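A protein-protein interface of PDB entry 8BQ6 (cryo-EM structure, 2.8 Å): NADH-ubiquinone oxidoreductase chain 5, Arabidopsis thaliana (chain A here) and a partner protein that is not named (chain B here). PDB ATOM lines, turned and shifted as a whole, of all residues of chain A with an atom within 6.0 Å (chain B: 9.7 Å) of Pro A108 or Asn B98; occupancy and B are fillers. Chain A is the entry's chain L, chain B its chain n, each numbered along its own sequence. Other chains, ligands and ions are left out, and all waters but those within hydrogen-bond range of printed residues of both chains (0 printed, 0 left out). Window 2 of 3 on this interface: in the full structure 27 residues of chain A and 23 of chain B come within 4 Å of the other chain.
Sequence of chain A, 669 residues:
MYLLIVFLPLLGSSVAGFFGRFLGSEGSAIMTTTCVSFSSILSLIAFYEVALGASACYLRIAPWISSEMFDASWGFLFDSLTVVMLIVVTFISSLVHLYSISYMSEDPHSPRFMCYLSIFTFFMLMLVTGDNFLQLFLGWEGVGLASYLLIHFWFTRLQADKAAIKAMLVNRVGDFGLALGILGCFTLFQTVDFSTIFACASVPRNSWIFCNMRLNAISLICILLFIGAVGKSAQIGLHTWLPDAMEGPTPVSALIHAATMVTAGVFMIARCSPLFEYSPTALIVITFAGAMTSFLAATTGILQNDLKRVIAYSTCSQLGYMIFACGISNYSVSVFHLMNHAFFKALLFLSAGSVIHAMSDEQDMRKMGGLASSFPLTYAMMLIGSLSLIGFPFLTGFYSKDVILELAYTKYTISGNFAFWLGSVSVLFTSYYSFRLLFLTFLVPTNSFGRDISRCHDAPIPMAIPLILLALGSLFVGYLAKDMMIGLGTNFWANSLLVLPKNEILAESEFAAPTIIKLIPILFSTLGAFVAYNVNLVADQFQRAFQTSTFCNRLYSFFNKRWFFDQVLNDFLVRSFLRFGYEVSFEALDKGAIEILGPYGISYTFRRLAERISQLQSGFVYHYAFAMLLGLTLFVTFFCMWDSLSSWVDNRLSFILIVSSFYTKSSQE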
ATOM      1  N   SER A  25      10.905  29.680 -30.859  1.00  0.00           N
ATOM      2  CA  SER A  25       9.968  28.924 -30.031  1.00  0.00           C
ATOM      3  C   SER A  25       8.730  28.516 -30.819  1.00  0.00           C
ATOM      4  O   SER A  25       8.231  27.394 -30.679  1.00  0.00           O
ATOM      5  CB  SER A  25       9.562  29.749 -28.810  1.00  0.00           C
ATOM      6  OG  SER A  25      10.666  29.998 -27.963  1.00  0.00           O
ATOM      7  N   MET A 104       4.907  25.035 -22.012  1.00  0.00           N
ATOM      8  CA  MET A 104       6.285  25.508 -21.967  1.00  0.00           C
ATOM      9  C   MET A 104       6.461  26.850 -22.666  1.00  0.00           C
ATOM     10  O   MET A 104       7.590  27.216 -23.011  1.00  0.00           O
ATOM     11  CB  MET A 104       7.228  24.471 -22.582  1.00  0.00           C
ATOM     12  CG  MET A 104       6.929  23.037 -22.190  1.00  0.00           C
ATOM     13  SD  MET A 104       7.719  22.517 -20.652  1.00  0.00           S
ATOM     14  CE  MET A 104       9.428  22.977 -20.931  1.00  0.00           C
ATOM     15  N   SER A 105       5.370  27.591 -22.877  1.00  0.00           N
ATOM     16  CA  SER A 105       5.450  28.858 -23.595  1.00  0.00           C
ATOM     17  C   SER A 105       6.370  29.849 -22.897  1.00  0.00           C
ATOM     18  O   SER A 105       7.128  30.568 -23.558  1.00  0.00           O
ATOM     19  CB  SER A 105       4.051  29.457 -23.755  1.00  0.00           C
ATOM     20  OG  SER A 105       3.434  29.672 -22.500  1.00  0.00           O
ATOM     21  N   GLU A 106       6.326  29.903 -21.574  1.00  0.00           N
ATOM     22  CA  GLU A 106       7.157  30.835 -20.830  1.00  0.00           C
ATOM     23  C   GLU A 106       8.551  30.289 -20.542  1.00  0.00           C
ATOM     24  O   GLU A 106       9.351  30.982 -19.908  1.00  0.00           O
ATOM     25  CB  GLU A 106       6.457  31.226 -19.527  1.00  0.00           C
ATOM     26  CG  GLU A 106       5.055  31.793 -19.738  1.00  0.00           C
ATOM     27  CD  GLU A 106       5.049  33.035 -20.617  1.00  0.00           C
ATOM     28  OE1 GLU A 106       5.807  33.979 -20.316  1.00  0.00           O
ATOM     29  OE2 GLU A 106       4.283  33.072 -21.604  1.00  0.00           O
ATOM     30  N   ASP A 107       8.858  29.075 -20.988  1.00  0.00           N
ATOM     31  CA  ASP A 107      10.184  28.522 -20.764  1.00  0.00           C
ATOM     32  C   ASP A 107      11.186  29.134 -21.741  1.00  0.00           C
ATOM     33  O   ASP A 107      10.865  29.339 -22.916  1.00  0.00           O
ATOM     34  CB  ASP A 107      10.165  27.002 -20.916  1.00  0.00           C
ATOM     35  CG  ASP A 107      11.424  26.346 -20.377  1.00  0.00           C
ATOM     36  OD1 ASP A 107      12.450  26.337 -21.089  1.00  0.00           O
ATOM     37  OD2 ASP A 107      11.397  25.864 -19.225  1.00  0.00           O
ATOM     38  N   PRO A 108      12.406  29.436 -21.288  1.00  0.00           N
ATOM     39  CA  PRO A 108      13.407  29.996 -22.209  1.00  0.00           C
ATOM     40  C   PRO A 108      13.862  29.031 -23.288  1.00  0.00           C
ATOM     41  O   PRO A 108      14.340  29.481 -24.335  1.00  0.00           O
ATOM     42  CB  PRO A 108      14.571  30.377 -21.281  1.00  0.00           C
ATOM     43  CG  PRO A 108      14.023  30.334 -19.902  1.00  0.00           C
ATOM     44  CD  PRO A 108      12.913  29.344 -19.911  1.00  0.00           C
ATOM     45  N   HIS A 109      13.740  27.724 -23.076  1.00  0.00           N
ATOM     46  CA  HIS A 109      14.386  26.733 -23.930  1.00  0.00           C
ATOM     47  C   HIS A 109      13.389  25.746 -24.515  1.00  0.00           C
ATOM     48  O   HIS A 109      13.640  24.541 -24.573  1.00  0.00           O
ATOM     49  CB  HIS A 109      15.466  25.993 -23.156  1.00  0.00           C
ATOM     50  CG  HIS A 109      16.517  26.897 -22.607  1.00  0.00           C
ATOM     51  ND1 HIS A 109      16.737  27.046 -21.255  1.00  0.00           N
ATOM     52  CD2 HIS A 109      17.388  27.726 -23.225  1.00  0.00           C
ATOM     53  CE1 HIS A 109      17.712  27.917 -21.066  1.00  0.00           C
ATOM     54  NE2 HIS A 109      18.121  28.346 -22.245  1.00  0.00           N
ATOM     55  N   SER A 110      12.246  26.259 -24.955  1.00  0.00           N
ATOM     56  CA  SER A 110      11.236  25.399 -25.559  1.00  0.00           C
ATOM     57  C   SER A 110      11.733  24.628 -26.781  1.00  0.00           C
ATOM     58  O   SER A 110      11.404  23.434 -26.885  1.00  0.00           O
ATOM     59  CB  SER A 110       9.999  26.240 -25.896  1.00  0.00           C
ATOM     60  OG  SER A 110       9.075  25.504 -26.673  1.00  0.00           O
ATOM     61  N   PRO A 111      12.487  25.211 -27.726  1.00  0.00           N
ATOM     62  CA  PRO A 111      12.871  24.424 -28.913  1.00  0.00           C
ATOM     63  C   PRO A 111      13.670  23.172 -28.597  1.00  0.00           C
ATOM     64  O   PRO A 111      13.486  22.144 -29.261  1.00  0.00           O
ATOM     65  CB  PRO A 111      13.686  25.424 -29.744  1.00  0.00           C
ATOM     66  CG  PRO A 111      13.201  26.744 -29.311  1.00  0.00           C
ATOM     67  CD  PRO A 111      12.935  26.610 -27.852  1.00  0.00           C
ATOM     68  N   TRP A 154      16.022  20.773 -17.104  1.00  0.00           N
ATOM     69  CA  TRP A 154      16.461  21.938 -16.332  1.00  0.00           C
ATOM     70  C   TRP A 154      17.800  21.592 -15.688  1.00  0.00           C
ATOM     71  O   TRP A 154      17.890  21.228 -14.513  1.00  0.00           O
ATOM     72  CB  TRP A 154      15.419  22.327 -15.292  1.00  0.00           C
ATOM     73  CG  TRP A 154      14.157  22.878 -15.875  1.00  0.00           C
ATOM     74  CD1 TRP A 154      14.052  23.861 -16.813  1.00  0.00           C
ATOM     75  CD2 TRP A 154      12.818  22.485 -15.557  1.00  0.00           C
ATOM     76  NE1 TRP A 154      12.732  24.105 -17.099  1.00  0.00           N
ATOM     77  CE2 TRP A 154      11.954  23.271 -16.342  1.00  0.00           C
ATOM     78  CE3 TRP A 154      12.266  21.542 -14.685  1.00  0.00           C
ATOM     79  CZ2 TRP A 154      10.572  23.146 -16.282  1.00  0.00           C
ATOM     80  CZ3 TRP A 154      10.893  21.422 -14.626  1.00  0.00           C
ATOM     81  CH2 TRP A 154      10.062  22.216 -15.421  1.00  0.00           C
ATOM     82  N   THR A 156      20.234  23.100 -14.524  1.00  0.00           N
ATOM     83  CA  THR A 156      20.725  23.851 -13.376  1.00  0.00           C
ATOM     84  C   THR A 156      20.249  23.292 -12.042  1.00  0.00           C
ATOM     85  O   THR A 156      20.840  23.618 -11.007  1.00  0.00           O
ATOM     86  CB  THR A 156      20.292  25.311 -13.494  1.00  0.00           C
ATOM     87  OG1 THR A 156      18.914  25.361 -13.883  1.00  0.00           O
ATOM     88  CG2 THR A 156      21.126  26.025 -14.535  1.00  0.00           C
ATOM     89  N   SER B  93      10.359  22.559  -5.200  1.00  0.00           N
ATOM     90  CA  SER B  93      10.254  21.941  -6.518  1.00  0.00           C
ATOM     91  C   SER B  93      10.728  22.872  -7.626  1.00  0.00           C
ATOM     92  O   SER B  93      11.113  22.402  -8.702  1.00  0.00           O
ATOM     93  CB  SER B  93       8.816  21.489  -6.788  1.00  0.00           C
ATOM     94  OG  SER B  93       7.869  22.487  -6.449  1.00  0.00           O
ATOM     95  N   LYS B  94      10.708  24.181  -7.394  1.00  0.00           N
ATOM     96  CA  LYS B  94      11.123  25.154  -8.393  1.00  0.00           C
ATOM     97  C   LYS B  94      12.496  25.738  -8.112  1.00  0.00           C
ATOM     98  O   LYS B  94      12.893  26.701  -8.775  1.00  0.00           O
ATOM     99  CB  LYS B  94      10.101  26.285  -8.477  1.00  0.00           C
ATOM    100  CG  LYS B  94       9.702  26.666  -9.882  1.00  0.00           C
ATOM    101  CD  LYS B  94       8.948  27.984  -9.869  1.00  0.00           C
ATOM    102  CE  LYS B  94       8.763  28.542 -11.267  1.00  0.00           C
ATOM    103  NZ  LYS B  94       9.950  28.304 -12.127  1.00  0.00           N
ATOM    104  N   PHE B  95      13.221  25.191  -7.146  1.00  0.00           N
ATOM    105  CA  PHE B  95      14.498  25.762  -6.760  1.00  0.00           C
ATOM    106  C   PHE B  95      15.551  25.487  -7.827  1.00  0.00           C
ATOM    107  O   PHE B  95      15.722  24.345  -8.266  1.00  0.00           O
ATOM    108  CB  PHE B  95      14.934  25.195  -5.416  1.00  0.00           C
ATOM    109  CG  PHE B  95      16.109  25.894  -4.830  1.00  0.00           C
ATOM    110  CD1 PHE B  95      16.124  27.272  -4.733  1.00  0.00           C
ATOM    111  CD2 PHE B  95      17.199  25.180  -4.382  1.00  0.00           C
ATOM    112  CE1 PHE B  95      17.203  27.925  -4.197  1.00  0.00           C
ATOM    113  CE2 PHE B  95      18.282  25.831  -3.844  1.00  0.00           C
ATOM    114  CZ  PHE B  95      18.283  27.205  -3.752  1.00  0.00           C
ATOM    115  N   CYS B  96      16.257  26.543  -8.234  1.00  0.00           N
ATOM    116  CA  CYS B  96      17.284  26.499  -9.274  1.00  0.00           C
ATOM    117  C   CYS B  96      16.719  26.136 -10.644  1.00  0.00           C
ATOM    118  O   CYS B  96      17.430  25.588 -11.487  1.00  0.00           O
ATOM    119  CB  CYS B  96      18.424  25.544  -8.905  1.00  0.00           C
ATOM    120  SG  CYS B  96      19.193  25.896  -7.312  1.00  0.00           S
ATOM    121  N   ARG B  97      15.450  26.446 -10.894  1.00  0.00           N
ATOM    122  CA  ARG B  97      14.880  26.281 -12.222  1.00  0.00           C
ATOM    123  C   ARG B  97      14.874  27.618 -12.948  1.00  0.00           C
ATOM    124  O   ARG B  97      14.376  28.617 -12.418  1.00  0.00           O
ATOM    125  CB  ARG B  97      13.463  25.723 -12.156  1.00  0.00           C
ATOM    126  CG  ARG B  97      12.912  25.449 -13.530  1.00  0.00           C
ATOM    127  CD  ARG B  97      11.414  25.529 -13.561  1.00  0.00           C
ATOM    128  NE  ARG B  97      10.782  24.344 -13.000  1.00  0.00           N
ATOM    129  CZ  ARG B  97       9.493  24.267 -12.708  1.00  0.00           C
ATOM    130  NH1 ARG B  97       8.684  25.298 -12.888  1.00  0.00           N
ATOM    131  NH2 ARG B  97       9.001  23.128 -12.232  1.00  0.00           N
ATOM    132  N   ASN B  98      15.409  27.621 -14.169  1.00  0.00           N
ATOM    133  CA  ASN B  98      15.651  28.810 -14.978  1.00  0.00           C
ATOM    134  C   ASN B  98      16.164  29.974 -14.139  1.00  0.00           C
ATOM    135  O   ASN B  98      15.539  31.041 -14.112  1.00  0.00           O
ATOM    136  CB  ASN B  98      14.379  29.216 -15.720  1.00  0.00           C
ATOM    137  CG  ASN B  98      13.903  28.140 -16.659  1.00  0.00           C
ATOM    138  OD1 ASN B  98      14.705  27.493 -17.328  1.00  0.00           O
ATOM    139  ND2 ASN B  98      12.595  27.933 -16.710  1.00  0.00           N
ATOM    140  N   PRO B  99      17.286  29.816 -13.444  1.00  0.00           N
ATOM    141  CA  PRO B  99      17.807  30.924 -12.643  1.00  0.00           C
ATOM    142  C   PRO B  99      18.451  31.989 -13.517  1.00  0.00           C
ATOM    143  O   PRO B  99      18.830  31.739 -14.665  1.00  0.00           O
ATOM    144  CB  PRO B  99      18.835  30.245 -11.737  1.00  0.00           C
ATOM    145  CG  PRO B  99      19.319  29.095 -12.543  1.00  0.00           C
ATOM    146  CD  PRO B  99      18.183  28.647 -13.414  1.00  0.00           C
ATOM    147  N   THR B 100      18.557  33.191 -12.963  1.00  0.00           N
ATOM    148  CA  THR B 100      19.131  34.298 -13.715  1.00  0.00           C
ATOM    149  C   THR B 100      20.626  34.069 -13.919  1.00  0.00           C
ATOM    150  O   THR B 100      21.288  33.470 -13.064  1.00  0.00           O
ATOM    151  CB  THR B 100      18.895  35.630 -12.998  1.00  0.00           C
ATOM    152  OG1 THR B 100      19.370  35.550 -11.649  1.00  0.00           O
ATOM    153  CG2 THR B 100      17.415  35.986 -12.997  1.00  0.00           C
ATOM    154  N   PRO B 101      21.188  34.518 -15.042  1.00  0.00           N
ATOM    155  CA  PRO B 101      22.606  34.279 -15.291  1.00  0.00           C
ATOM    156  C   PRO B 101      23.460  35.000 -14.266  1.00  0.00           C
ATOM    157  O   PRO B 101      23.093  36.085 -13.782  1.00  0.00           O
ATOM    158  CB  PRO B 101      22.822  34.859 -16.700  1.00  0.00           C
ATOM    159  CG  PRO B 101      21.478  35.029 -17.274  1.00  0.00           C
ATOM    160  CD  PRO B 101      20.534  35.228 -16.151  1.00  0.00           C
ATOM    161  N   PRO B 102      24.603  34.434 -13.895  1.00  0.00           N
ATOM    162  CA  PRO B 102      25.540  35.176 -13.048  1.00  0.00           C
ATOM    163  C   PRO B 102      26.172  36.322 -13.820  1.00  0.00           C
ATOM    164  O   PRO B 102      26.299  36.282 -15.045  1.00  0.00           O
ATOM    165  CB  PRO B 102      26.582  34.124 -12.656  1.00  0.00           C
ATOM    166  CG  PRO B 102      26.502  33.089 -13.710  1.00  0.00           C
ATOM    167  CD  PRO B 102      25.109  33.102 -14.266  1.00  0.00           C
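OD2 of Asp A107 sits at hydrogen-bond distance from ND2 of Asn B98 (3.5 Å).
The backbone carbonyl oxygen of Cys B96 is in hydrogen-bond range of the side-chain hydroxyl of Thr A156.
The side-chain carboxylate of Asp A107 is in hydrogen-bond range of the backbone NH of His A109, at 2.7 Å.
The side-chain carboxylate (OD2) of Asp A107 is in hydrogen-bond range of the indole nitrogen (NE1) of Trp A154.
Among the printed residues, pairs that only touch across the chains: Trp A154 with Arg B97, Thr A156 with Pro B99, Pro A108 with Asn B98 and Trp A154 with Asn B98.
Asn B98 touches three residues of chain A.
No residue of chain B comes within 4 Å of His A109.
Of the printed residues of chain A, Arg B97 touches Trp A154.
Of the printed residues of chain A, Pro B99 touches Thr A156.
Ser A110 touches none of the printed residues of chain B.
Thr B100 touches none of the printed residues of chain A.
The nearest residue of chain B that does not touch Pro A108 is Pro B99 (7.2 Å).
Hydrophobic or aromatic side chains of chain B within 4 Å of the printed part of chain A: Pro B99.
Printed residues of chain A that touch a printed residue of chain B: Asp A107, Pro A108, Trp A154 and Thr A156.
Hydrophobic or aromatic side chains of chain A within 4 Å of the printed part of chain B: Pro A108 and Trp A154.
Among the printed residues, 6 pairs touch across the chains.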
